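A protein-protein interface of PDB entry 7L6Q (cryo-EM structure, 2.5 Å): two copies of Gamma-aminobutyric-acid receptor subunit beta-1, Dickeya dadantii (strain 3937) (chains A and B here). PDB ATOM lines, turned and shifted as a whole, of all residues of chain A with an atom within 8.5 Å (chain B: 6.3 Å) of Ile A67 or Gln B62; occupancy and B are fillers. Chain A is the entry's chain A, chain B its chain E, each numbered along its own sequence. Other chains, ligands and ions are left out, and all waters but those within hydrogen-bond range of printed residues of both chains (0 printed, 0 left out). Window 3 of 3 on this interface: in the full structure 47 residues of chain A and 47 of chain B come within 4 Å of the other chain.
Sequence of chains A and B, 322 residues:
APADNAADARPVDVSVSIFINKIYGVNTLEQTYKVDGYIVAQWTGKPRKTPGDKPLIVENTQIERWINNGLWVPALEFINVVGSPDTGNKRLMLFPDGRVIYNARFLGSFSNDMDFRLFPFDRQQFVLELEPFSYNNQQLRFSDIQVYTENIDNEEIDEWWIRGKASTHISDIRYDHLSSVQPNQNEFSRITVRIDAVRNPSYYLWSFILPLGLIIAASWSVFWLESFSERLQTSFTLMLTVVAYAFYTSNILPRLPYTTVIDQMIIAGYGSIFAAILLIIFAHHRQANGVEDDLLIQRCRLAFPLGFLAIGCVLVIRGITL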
ATOM      1  N   VAL A  58       1.478  10.670 -18.697  1.00  0.00           N
ATOM      2  CA  VAL A  58       2.008  10.856 -20.039  1.00  0.00           C
ATOM      3  C   VAL A  58       3.454  10.391 -20.022  1.00  0.00           C
ATOM      4  O   VAL A  58       4.302  11.020 -19.381  1.00  0.00           O
ATOM      5  CB  VAL A  58       1.912  12.315 -20.488  1.00  0.00           C
ATOM      6  CG1 VAL A  58       2.555  12.492 -21.825  1.00  0.00           C
ATOM      7  CG2 VAL A  58       0.473  12.744 -20.539  1.00  0.00           C
ATOM      8  N   ASN A  60       7.035   8.474 -22.079  1.00  0.00           N
ATOM      9  CA  ASN A  60       8.226   8.987 -22.750  1.00  0.00           C
ATOM     10  C   ASN A  60       7.995   9.823 -24.000  1.00  0.00           C
ATOM     11  O   ASN A  60       8.286  11.022 -23.999  1.00  0.00           O
ATOM     12  CB  ASN A  60       9.128   7.818 -23.117  1.00  0.00           C
ATOM     13  CG  ASN A  60       9.221   6.804 -22.020  1.00  0.00           C
ATOM     14  OD1 ASN A  60      10.011   6.949 -21.098  1.00  0.00           O
ATOM     15  ND2 ASN A  60       8.410   5.764 -22.106  1.00  0.00           N
ATOM     16  N   THR A  61       7.479   9.229 -25.067  1.00  0.00           N
ATOM     17  CA  THR A  61       7.364   9.967 -26.316  1.00  0.00           C
ATOM     18  C   THR A  61       6.078  10.763 -26.417  1.00  0.00           C
ATOM     19  O   THR A  61       5.954  11.593 -27.320  1.00  0.00           O
ATOM     20  CB  THR A  61       7.460   9.026 -27.514  1.00  0.00           C
ATOM     21  OG1 THR A  61       6.412   8.055 -27.445  1.00  0.00           O
ATOM     22  CG2 THR A  61       8.797   8.322 -27.519  1.00  0.00           C
ATOM     23  N   GLN A  62       5.125  10.535 -25.525  1.00  0.00           N
ATOM     24  CA  GLN A  62       3.920  11.342 -25.512  1.00  0.00           C
ATOM     25  C   GLN A  62       4.131  12.696 -24.859  1.00  0.00           C
ATOM     26  O   GLN A  62       3.273  13.569 -25.000  1.00  0.00           O
ATOM     27  CB  GLN A  62       2.802  10.594 -24.798  1.00  0.00           C
ATOM     28  CG  GLN A  62       2.361   9.376 -25.532  1.00  0.00           C
ATOM     29  CD  GLN A  62       1.968   9.704 -26.938  1.00  0.00           C
ATOM     30  OE1 GLN A  62       1.129  10.568 -27.170  1.00  0.00           O
ATOM     31  NE2 GLN A  62       2.584   9.030 -27.896  1.00  0.00           N
ATOM     32  N   ILE A  63       5.238  12.885 -24.140  1.00  0.00           N
ATOM     33  CA  ILE A  63       5.529  14.190 -23.563  1.00  0.00           C
ATOM     34  C   ILE A  63       5.734  15.218 -24.661  1.00  0.00           C
ATOM     35  O   ILE A  63       5.232  16.343 -24.583  1.00  0.00           O
ATOM     36  CB  ILE A  63       6.754  14.108 -22.640  1.00  0.00           C
ATOM     37  CG1 ILE A  63       6.465  13.210 -21.452  1.00  0.00           C
ATOM     38  CG2 ILE A  63       7.126  15.472 -22.150  1.00  0.00           C
ATOM     39  CD1 ILE A  63       7.608  13.123 -20.494  1.00  0.00           C
ATOM     40  N   GLU A  64       6.471  14.843 -25.706  1.00  0.00           N
ATOM     41  CA  GLU A  64       6.775  15.787 -26.773  1.00  0.00           C
ATOM     42  C   GLU A  64       5.520  16.256 -27.485  1.00  0.00           C
ATOM     43  O   GLU A  64       5.489  17.373 -28.010  1.00  0.00           O
ATOM     44  CB  GLU A  64       7.737  15.156 -27.771  1.00  0.00           C
ATOM     45  CG  GLU A  64       8.926  16.024 -28.089  1.00  0.00           C
ATOM     46  CD  GLU A  64       9.808  16.250 -26.881  1.00  0.00           C
ATOM     47  OE1 GLU A  64       9.845  15.366 -25.999  1.00  0.00           O
ATOM     48  OE2 GLU A  64      10.460  17.312 -26.808  1.00  0.00           O
ATOM     49  N   ARG A  65       4.481  15.428 -27.520  1.00  0.00           N
ATOM     50  CA  ARG A  65       3.250  15.861 -28.160  1.00  0.00           C
ATOM     51  C   ARG A  65       2.498  16.862 -27.299  1.00  0.00           C
ATOM     52  O   ARG A  65       1.740  17.680 -27.824  1.00  0.00           O
ATOM     53  CB  ARG A  65       2.365  14.661 -28.475  1.00  0.00           C
ATOM     54  CG  ARG A  65       1.360  14.942 -29.564  1.00  0.00           C
ATOM     55  CD  ARG A  65       0.433  13.773 -29.792  1.00  0.00           C
ATOM     56  NE  ARG A  65      -0.545  13.647 -28.721  1.00  0.00           N
ATOM     57  CZ  ARG A  65      -1.610  12.859 -28.780  1.00  0.00           C
ATOM     58  NH1 ARG A  65      -1.832  12.128 -29.862  1.00  0.00           N
ATOM     59  NH2 ARG A  65      -2.454  12.803 -27.760  1.00  0.00           N
ATOM     60  N   TRP A  66       2.681  16.806 -25.982  1.00  0.00           N
ATOM     61  CA  TRP A  66       2.050  17.786 -25.109  1.00  0.00           C
ATOM     62  C   TRP A  66       2.777  19.118 -25.124  1.00  0.00           C
ATOM     63  O   TRP A  66       2.138  20.167 -25.003  1.00  0.00           O
ATOM     64  CB  TRP A  66       1.975  17.253 -23.683  1.00  0.00           C
ATOM     65  CG  TRP A  66       0.866  16.301 -23.478  1.00  0.00           C
ATOM     66  CD1 TRP A  66       0.867  14.979 -23.768  1.00  0.00           C
ATOM     67  CD2 TRP A  66      -0.419  16.593 -22.937  1.00  0.00           C
ATOM     68  NE1 TRP A  66      -0.338  14.424 -23.442  1.00  0.00           N
ATOM     69  CE2 TRP A  66      -1.145  15.398 -22.927  1.00  0.00           C
ATOM     70  CE3 TRP A  66      -1.025  17.752 -22.460  1.00  0.00           C
ATOM     71  CZ2 TRP A  66      -2.444  15.327 -22.461  1.00  0.00           C
ATOM     72  CZ3 TRP A  66      -2.311  17.678 -21.998  1.00  0.00           C
ATOM     73  CH2 TRP A  66      -3.008  16.477 -22.001  1.00  0.00           C
ATOM     74  N   ILE A  67       4.102  19.102 -25.258  1.00  0.00           N
ATOM     75  CA  ILE A  67       4.851  20.350 -25.328  1.00  0.00           C
ATOM     76  C   ILE A  67       4.472  21.124 -26.581  1.00  0.00           C
ATOM     77  O   ILE A  67       4.301  22.347 -26.543  1.00  0.00           O
ATOM     78  CB  ILE A  67       6.361  20.072 -25.266  1.00  0.00           C
ATOM     79  CG1 ILE A  67       6.722  19.439 -23.932  1.00  0.00           C
ATOM     80  CG2 ILE A  67       7.135  21.346 -25.440  1.00  0.00           C
ATOM     81  CD1 ILE A  67       8.186  19.222 -23.761  1.00  0.00           C
ATOM     82  N   ASN A  68       4.326  20.425 -27.708  1.00  0.00           N
ATOM     83  CA  ASN A  68       3.948  21.095 -28.947  1.00  0.00           C
ATOM     84  C   ASN A  68       2.592  21.771 -28.834  1.00  0.00           C
ATOM     85  O   ASN A  68       2.333  22.757 -29.530  1.00  0.00           O
ATOM     86  CB  ASN A  68       3.939  20.103 -30.104  1.00  0.00           C
ATOM     87  CG  ASN A  68       5.313  19.583 -30.429  1.00  0.00           C
ATOM     88  OD1 ASN A  68       6.312  20.096 -29.937  1.00  0.00           O
ATOM     89  ND2 ASN A  68       5.375  18.563 -31.271  1.00  0.00           N
ATOM     90  N   ASN A  69       1.718  21.268 -27.973  1.00  0.00           N
ATOM     91  CA  ASN A  69       0.408  21.869 -27.782  1.00  0.00           C
ATOM     92  C   ASN A  69       0.410  22.967 -26.733  1.00  0.00           C
ATOM     93  O   ASN A  69      -0.657  23.500 -26.417  1.00  0.00           O
ATOM     94  CB  ASN A  69      -0.617  20.804 -27.406  1.00  0.00           C
ATOM     95  CG  ASN A  69      -0.906  19.859 -28.542  1.00  0.00           C
ATOM     96  OD1 ASN A  69      -0.647  20.174 -29.700  1.00  0.00           O
ATOM     97  ND2 ASN A  69      -1.450  18.695 -28.221  1.00  0.00           N
ATOM     98  N   GLY A  70       1.562  23.303 -26.175  1.00  0.00           N
ATOM     99  CA  GLY A  70       1.677  24.441 -25.297  1.00  0.00           C
ATOM    100  C   GLY A  70       1.811  24.147 -23.823  1.00  0.00           C
ATOM    101  O   GLY A  70       1.571  25.047 -23.014  1.00  0.00           O
ATOM    102  N   LEU A  71       2.184  22.932 -23.445  1.00  0.00           N
ATOM    103  CA  LEU A  71       2.402  22.627 -22.040  1.00  0.00           C
ATOM    104  C   LEU A  71       3.769  23.137 -21.618  1.00  0.00           C
ATOM    105  O   LEU A  71       4.757  22.954 -22.332  1.00  0.00           O
ATOM    106  CB  LEU A  71       2.298  21.127 -21.793  1.00  0.00           C
ATOM    107  CG  LEU A  71       2.431  20.733 -20.330  1.00  0.00           C
ATOM    108  CD1 LEU A  71       1.289  21.323 -19.550  1.00  0.00           C
ATOM    109  CD2 LEU A  71       2.451  19.239 -20.193  1.00  0.00           C
ATOM    110  N   TRP A  72       3.826  23.779 -20.460  1.00  0.00           N
ATOM    111  CA  TRP A  72       5.055  24.387 -19.970  1.00  0.00           C
ATOM    112  C   TRP A  72       5.819  23.365 -19.141  1.00  0.00           C
ATOM    113  O   TRP A  72       5.436  23.065 -18.007  1.00  0.00           O
ATOM    114  CB  TRP A  72       4.738  25.635 -19.155  1.00  0.00           C
ATOM    115  CG  TRP A  72       5.943  26.384 -18.731  1.00  0.00           C
ATOM    116  CD1 TRP A  72       6.735  27.156 -19.514  1.00  0.00           C
ATOM    117  CD2 TRP A  72       6.497  26.443 -17.418  1.00  0.00           C
ATOM    118  NE1 TRP A  72       7.754  27.690 -18.774  1.00  0.00           N
ATOM    119  CE2 TRP A  72       7.627  27.265 -17.480  1.00  0.00           C
ATOM    120  CE3 TRP A  72       6.147  25.875 -16.195  1.00  0.00           C
ATOM    121  CZ2 TRP A  72       8.409  27.534 -16.372  1.00  0.00           C
ATOM    122  CZ3 TRP A  72       6.924  26.145 -15.099  1.00  0.00           C
ATOM    123  CH2 TRP A  72       8.041  26.964 -15.191  1.00  0.00           C
ATOM    124  N   VAL A  73       6.895  22.828 -19.703  1.00  0.00           N
ATOM    125  CA  VAL A  73       7.748  21.880 -18.994  1.00  0.00           C
ATOM    126  C   VAL A  73       9.170  22.423 -18.969  1.00  0.00           C
ATOM    127  O   VAL A  73       9.920  22.226 -19.934  1.00  0.00           O
ATOM    128  CB  VAL A  73       7.700  20.492 -19.643  1.00  0.00           C
ATOM    129  CG1 VAL A  73       8.588  19.538 -18.893  1.00  0.00           C
ATOM    130  CG2 VAL A  73       6.285  19.978 -19.664  1.00  0.00           C
ATOM    131  N   PRO A  74       9.580  23.114 -17.909  1.00  0.00           N
ATOM    132  CA  PRO A  74      10.916  23.712 -17.894  1.00  0.00           C
ATOM    133  C   PRO A  74      12.003  22.655 -17.950  1.00  0.00           C
ATOM    134  O   PRO A  74      11.867  21.567 -17.394  1.00  0.00           O
ATOM    135  CB  PRO A  74      10.942  24.472 -16.568  1.00  0.00           C
ATOM    136  CG  PRO A  74       9.973  23.769 -15.728  1.00  0.00           C
ATOM    137  CD  PRO A  74       8.873  23.342 -16.645  1.00  0.00           C
ATOM    138  N   ALA A  75      13.092  22.990 -18.629  1.00  0.00           N
ATOM    139  CA  ALA A  75      14.230  22.096 -18.756  1.00  0.00           C
ATOM    140  C   ALA A  75      15.196  22.363 -17.615  1.00  0.00           C
ATOM    141  O   ALA A  75      15.664  23.491 -17.446  1.00  0.00           O
ATOM    142  CB  ALA A  75      14.921  22.290 -20.101  1.00  0.00           C
ATOM    143  N   LYS A  90      10.914   8.838 -18.883  1.00  0.00           N
ATOM    144  CA  LYS A  90      10.345  10.087 -18.413  1.00  0.00           C
ATOM    145  C   LYS A  90       8.859   9.894 -18.172  1.00  0.00           C
ATOM    146  O   LYS A  90       8.257   8.927 -18.635  1.00  0.00           O
ATOM    147  CB  LYS A  90      10.565  11.215 -19.420  1.00  0.00           C
ATOM    148  CG  LYS A  90      11.991  11.402 -19.831  1.00  0.00           C
ATOM    149  CD  LYS A  90      12.164  12.711 -20.557  1.00  0.00           C
ATOM    150  CE  LYS A  90      11.319  12.756 -21.801  1.00  0.00           C
ATOM    151  NZ  LYS A  90      11.784  11.761 -22.787  1.00  0.00           N
ATOM    152  N   LEU A  92       5.132  12.396 -17.053  1.00  0.00           N
ATOM    153  CA  LEU A  92       4.396  13.524 -16.509  1.00  0.00           C
ATOM    154  C   LEU A  92       3.124  13.015 -15.854  1.00  0.00           C
ATOM    155  O   LEU A  92       2.538  12.025 -16.297  1.00  0.00           O
ATOM    156  CB  LEU A  92       4.029  14.536 -17.585  1.00  0.00           C
ATOM    157  CG  LEU A  92       5.092  15.500 -18.082  1.00  0.00           C
ATOM    158  CD1 LEU A  92       4.512  16.332 -19.179  1.00  0.00           C
ATOM    159  CD2 LEU A  92       5.549  16.382 -16.960  1.00  0.00           C
ATOM    160  N   TYR A 102       6.940  16.002 -12.744  1.00  0.00           N
ATOM    161  CA  TYR A 102       7.859  15.534 -13.767  1.00  0.00           C
ATOM    162  C   TYR A 102       8.840  14.570 -13.124  1.00  0.00           C
ATOM    163  O   TYR A 102       9.442  14.891 -12.097  1.00  0.00           O
ATOM    164  CB  TYR A 102       8.594  16.706 -14.408  1.00  0.00           C
ATOM    165  CG  TYR A 102       9.635  16.312 -15.414  1.00  0.00           C
ATOM    166  CD1 TYR A 102       9.291  16.048 -16.720  1.00  0.00           C
ATOM    167  CD2 TYR A 102      10.963  16.227 -15.062  1.00  0.00           C
ATOM    168  CE1 TYR A 102      10.237  15.695 -17.639  1.00  0.00           C
ATOM    169  CE2 TYR A 102      11.915  15.876 -15.974  1.00  0.00           C
ATOM    170  CZ  TYR A 102      11.547  15.611 -17.262  1.00  0.00           C
ATOM    171  OH  TYR A 102      12.502  15.258 -18.180  1.00  0.00           O
ATOM    172  N   VAL B  58      12.343  29.438 -26.423  1.00  0.00           N
ATOM    173  CA  VAL B  58      12.072  28.236 -27.196  1.00  0.00           C
ATOM    174  C   VAL B  58      13.195  27.253 -26.913  1.00  0.00           C
ATOM    175  O   VAL B  58      14.341  27.491 -27.306  1.00  0.00           O
ATOM    176  CB  VAL B  58      11.975  28.536 -28.693  1.00  0.00           C
ATOM    177  CG1 VAL B  58      11.798  27.270 -29.468  1.00  0.00           C
ATOM    178  CG2 VAL B  58      10.834  29.475 -28.957  1.00  0.00           C
ATOM    179  N   GLU B  59      12.875  26.155 -26.243  1.00  0.00           N
ATOM    180  CA  GLU B  59      13.879  25.199 -25.802  1.00  0.00           C
ATOM    181  C   GLU B  59      14.044  24.065 -26.813  1.00  0.00           C
ATOM    182  O   GLU B  59      13.576  24.142 -27.951  1.00  0.00           O
ATOM    183  CB  GLU B  59      13.538  24.693 -24.409  1.00  0.00           C
ATOM    184  CG  GLU B  59      13.979  25.652 -23.336  1.00  0.00           C
ATOM    185  CD  GLU B  59      13.628  25.185 -21.954  1.00  0.00           C
ATOM    186  OE1 GLU B  59      12.733  24.329 -21.826  1.00  0.00           O
ATOM    187  OE2 GLU B  59      14.249  25.674 -20.991  1.00  0.00           O
ATOM    188  N   ASN B  60      14.706  22.992 -26.383  1.00  0.00           N
ATOM    189  CA  ASN B  60      15.396  22.035 -27.243  1.00  0.00           C
ATOM    190  C   ASN B  60      14.653  21.584 -28.492  1.00  0.00           C
ATOM    191  O   ASN B  60      15.081  21.891 -29.607  1.00  0.00           O
ATOM    192  CB  ASN B  60      15.752  20.802 -26.425  1.00  0.00           C
ATOM    193  CG  ASN B  60      16.270  21.151 -25.066  1.00  0.00           C
ATOM    194  OD1 ASN B  60      17.447  21.435 -24.898  1.00  0.00           O
ATOM    195  ND2 ASN B  60      15.393  21.135 -24.078  1.00  0.00           N
ATOM    196  N   THR B  61      13.550  20.863 -28.340  1.00  0.00           N
ATOM    197  CA  THR B  61      12.886  20.307 -29.510  1.00  0.00           C
ATOM    198  C   THR B  61      11.900  21.268 -30.143  1.00  0.00           C
ATOM    199  O   THR B  61      11.434  21.007 -31.254  1.00  0.00           O
ATOM    200  CB  THR B  61      12.161  19.011 -29.159  1.00  0.00           C
ATOM    201  OG1 THR B  61      11.185  19.269 -28.146  1.00  0.00           O
ATOM    202  CG2 THR B  61      13.145  17.981 -28.658  1.00  0.00           C
ATOM    203  N   GLN B  62      11.572  22.364 -29.474  1.00  0.00           N
ATOM    204  CA  GLN B  62      10.717  23.368 -30.078  1.00  0.00           C
ATOM    205  C   GLN B  62      11.461  24.256 -31.057  1.00  0.00           C
ATOM    206  O   GLN B  62      10.817  24.979 -31.821  1.00  0.00           O
ATOM    207  CB  GLN B  62      10.072  24.221 -28.995  1.00  0.00           C
ATOM    208  CG  GLN B  62       9.116  23.456 -28.149  1.00  0.00           C
ATOM    209  CD  GLN B  62       8.073  22.782 -28.984  1.00  0.00           C
ATOM    210  OE1 GLN B  62       7.393  23.425 -29.778  1.00  0.00           O
ATOM    211  NE2 GLN B  62       7.948  21.473 -28.829  1.00  0.00           N
ATOM    212  N   ILE B  63      12.793  24.232 -31.045  1.00  0.00           N
ATOM    213  CA  ILE B  63      13.555  25.002 -32.020  1.00  0.00           C
ATOM    214  C   ILE B  63      13.284  24.490 -33.423  1.00  0.00           C
ATOM    215  O   ILE B  63      13.091  25.271 -34.360  1.00  0.00           O
ATOM    216  CB  ILE B  63      15.054  24.954 -31.690  1.00  0.00           C
ATOM    217  CG1 ILE B  63      15.326  25.628 -30.359  1.00  0.00           C
ATOM    218  CG2 ILE B  63      15.844  25.637 -32.762  1.00  0.00           C
ATOM    219  CD1 ILE B  63      16.777  25.649 -30.003  1.00  0.00           C
ATOM    220  N   GLU B  64      13.255  23.167 -33.588  1.00  0.00           N
ATOM    221  CA  GLU B  64      13.069  22.591 -34.912  1.00  0.00           C
ATOM    222  C   GLU B  64      11.723  22.963 -35.503  1.00  0.00           C
ATOM    223  O   GLU B  64      11.584  23.036 -36.727  1.00  0.00           O
ATOM    224  CB  GLU B  64      13.212  21.076 -34.847  1.00  0.00           C
ATOM    225  CG  GLU B  64      14.151  20.517 -35.884  1.00  0.00           C
ATOM    226  CD  GLU B  64      15.573  20.991 -35.681  1.00  0.00           C
ATOM    227  OE1 GLU B  64      15.949  21.266 -34.523  1.00  0.00           O
ATOM    228  OE2 GLU B  64      16.315  21.095 -36.680  1.00  0.00           O
ATOM    229  N   ARG B  65      10.719  23.195 -34.663  1.00  0.00           N
ATOM    230  CA  ARG B  65       9.426  23.591 -35.194  1.00  0.00           C
ATOM    231  C   ARG B  65       9.438  25.032 -35.671  1.00  0.00           C
ATOM    232  O   ARG B  65       8.655  25.397 -36.552  1.00  0.00           O
ATOM    233  CB  ARG B  65       8.337  23.387 -34.147  1.00  0.00           C
ATOM    234  CG  ARG B  65       6.958  23.269 -34.747  1.00  0.00           C
ATOM    235  CD  ARG B  65       5.888  23.163 -33.688  1.00  0.00           C
ATOM    236  NE  ARG B  65       5.652  24.444 -33.036  1.00  0.00           N
ATOM    237  CZ  ARG B  65       4.621  24.689 -32.238  1.00  0.00           C
ATOM    238  NH1 ARG B  65       3.731  23.739 -31.998  1.00  0.00           N
ATOM    239  NH2 ARG B  65       4.479  25.884 -31.684  1.00  0.00           N
ATOM    240  N   TRP B  66      10.301  25.867 -35.098  1.00  0.00           N
ATOM    241  CA  TRP B  66      10.416  27.243 -35.563  1.00  0.00           C
ATOM    242  C   TRP B  66      11.215  27.345 -36.850  1.00  0.00           C
ATOM    243  O   TRP B  66      10.921  28.205 -37.685  1.00  0.00           O
ATOM    244  CB  TRP B  66      11.053  28.114 -34.487  1.00  0.00           C
ATOM    245  CG  TRP B  66      10.104  28.512 -33.428  1.00  0.00           C
ATOM    246  CD1 TRP B  66       9.739  27.781 -32.349  1.00  0.00           C
ATOM    247  CD2 TRP B  66       9.392  29.741 -33.341  1.00  0.00           C
ATOM    248  NE1 TRP B  66       8.841  28.476 -31.591  1.00  0.00           N
ATOM    249  CE2 TRP B  66       8.613  29.688 -32.180  1.00  0.00           C
ATOM    250  CE3 TRP B  66       9.340  30.884 -34.134  1.00  0.00           C
ATOM    251  CZ2 TRP B  66       7.791  30.729 -31.794  1.00  0.00           C
ATOM    252  CZ3 TRP B  66       8.524  31.915 -33.748  1.00  0.00           C
ATOM    253  CH2 TRP B  66       7.760  31.833 -32.589  1.00  0.00           C
ATOM    254  N   ILE B  67      12.227  26.498 -37.024  1.00  0.00           N
ATOM    255  CA  ILE B  67      13.000  26.516 -38.259  1.00  0.00           C
ATOM    256  C   ILE B  67      12.124  26.120 -39.437  1.00  0.00           C
ATOM    257  O   ILE B  67      12.196  26.725 -40.512  1.00  0.00           O
ATOM    258  CB  ILE B  67      14.230  25.604 -38.134  1.00  0.00           C
ATOM    259  CG1 ILE B  67      15.158  26.124 -37.048  1.00  0.00           C
ATOM    260  CG2 ILE B  67      14.971  25.542 -39.437  1.00  0.00           C
ATOM    261  CD1 ILE B  67      16.421  25.342 -36.928  1.00  0.00           C
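OG1 of Thr B61 is in hydrogen-bond range of OE2 of Glu A64. The side-chain amide oxygen (OD1) of Asn A68 sits at hydrogen-bond distance from the side-chain amide nitrogen (NE2) of Gln B62 (2.4 Å). O of Asn A68 is in hydrogen-bond range of NH1 of Arg B65, 3.0 Å away. The side-chain carboxylate (OE1) of Glu B59 lies close to the backbone NH (N) of Ala A75 (3.5 Å).
Of the 10 printed residues of chain B, 4 touch a printed residue of chain A. Hydrophobic or aromatic side chains of chain A within 4 Å of the printed part of chain B: Ile A67 and Ala A75. Among the printed residues, 6 pairs touch across the chains. Among the printed residues, no Asp or Glu carboxylate lies within 4 Å of a Lys or Arg side-chain nitrogen of the other chain.
Glu A64 touches Thr B61, but with the chains exchanged Thr A61 does not touch Glu B64 (14.1 Å). Ile A67 touches Gln B62, but with the chains exchanged Gln A62 does not touch Ile B67 (19.8 Å). Of the 6 pairs that touch across the chains among the printed residues, none has its exchanged pair printed and touching as well.
Of chain B, only Gln B62 (3.5 Å) comes within 4 Å of Ile A67. Printed residues of chain A within 4 Å of Gln B62: Ile A67 and Asn A68. Of the printed residues of chain A, Thr B61 touches Glu A64. Printed residues of chain B within 4 Å of Val A73: Glu B59 (3.99 Å). Printed residues of chain A within 4 Å of Glu B59: Val A73 (3.99 Å) and Ala A75 (3.5 Å). Leu A92 touches none of the printed residues of chain B. The nearest residue of chain B that does not touch Ile A67 is Thr B61 (5.3 Å). The nearest residue of chain A that does not touch Gln B62 is Glu A64 (4.9 Å).
Among the printed residues, pairs that only touch across the chains: Ile A67 with Gln B62 (3.5 Å) and Val A73 with Glu B59 (3.99 Å).
The backbone carbonyl oxygen (O) of Glu A64 lies close to the side-chain amide oxygen (OD1) of Asn A68, 3.4 Å away.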
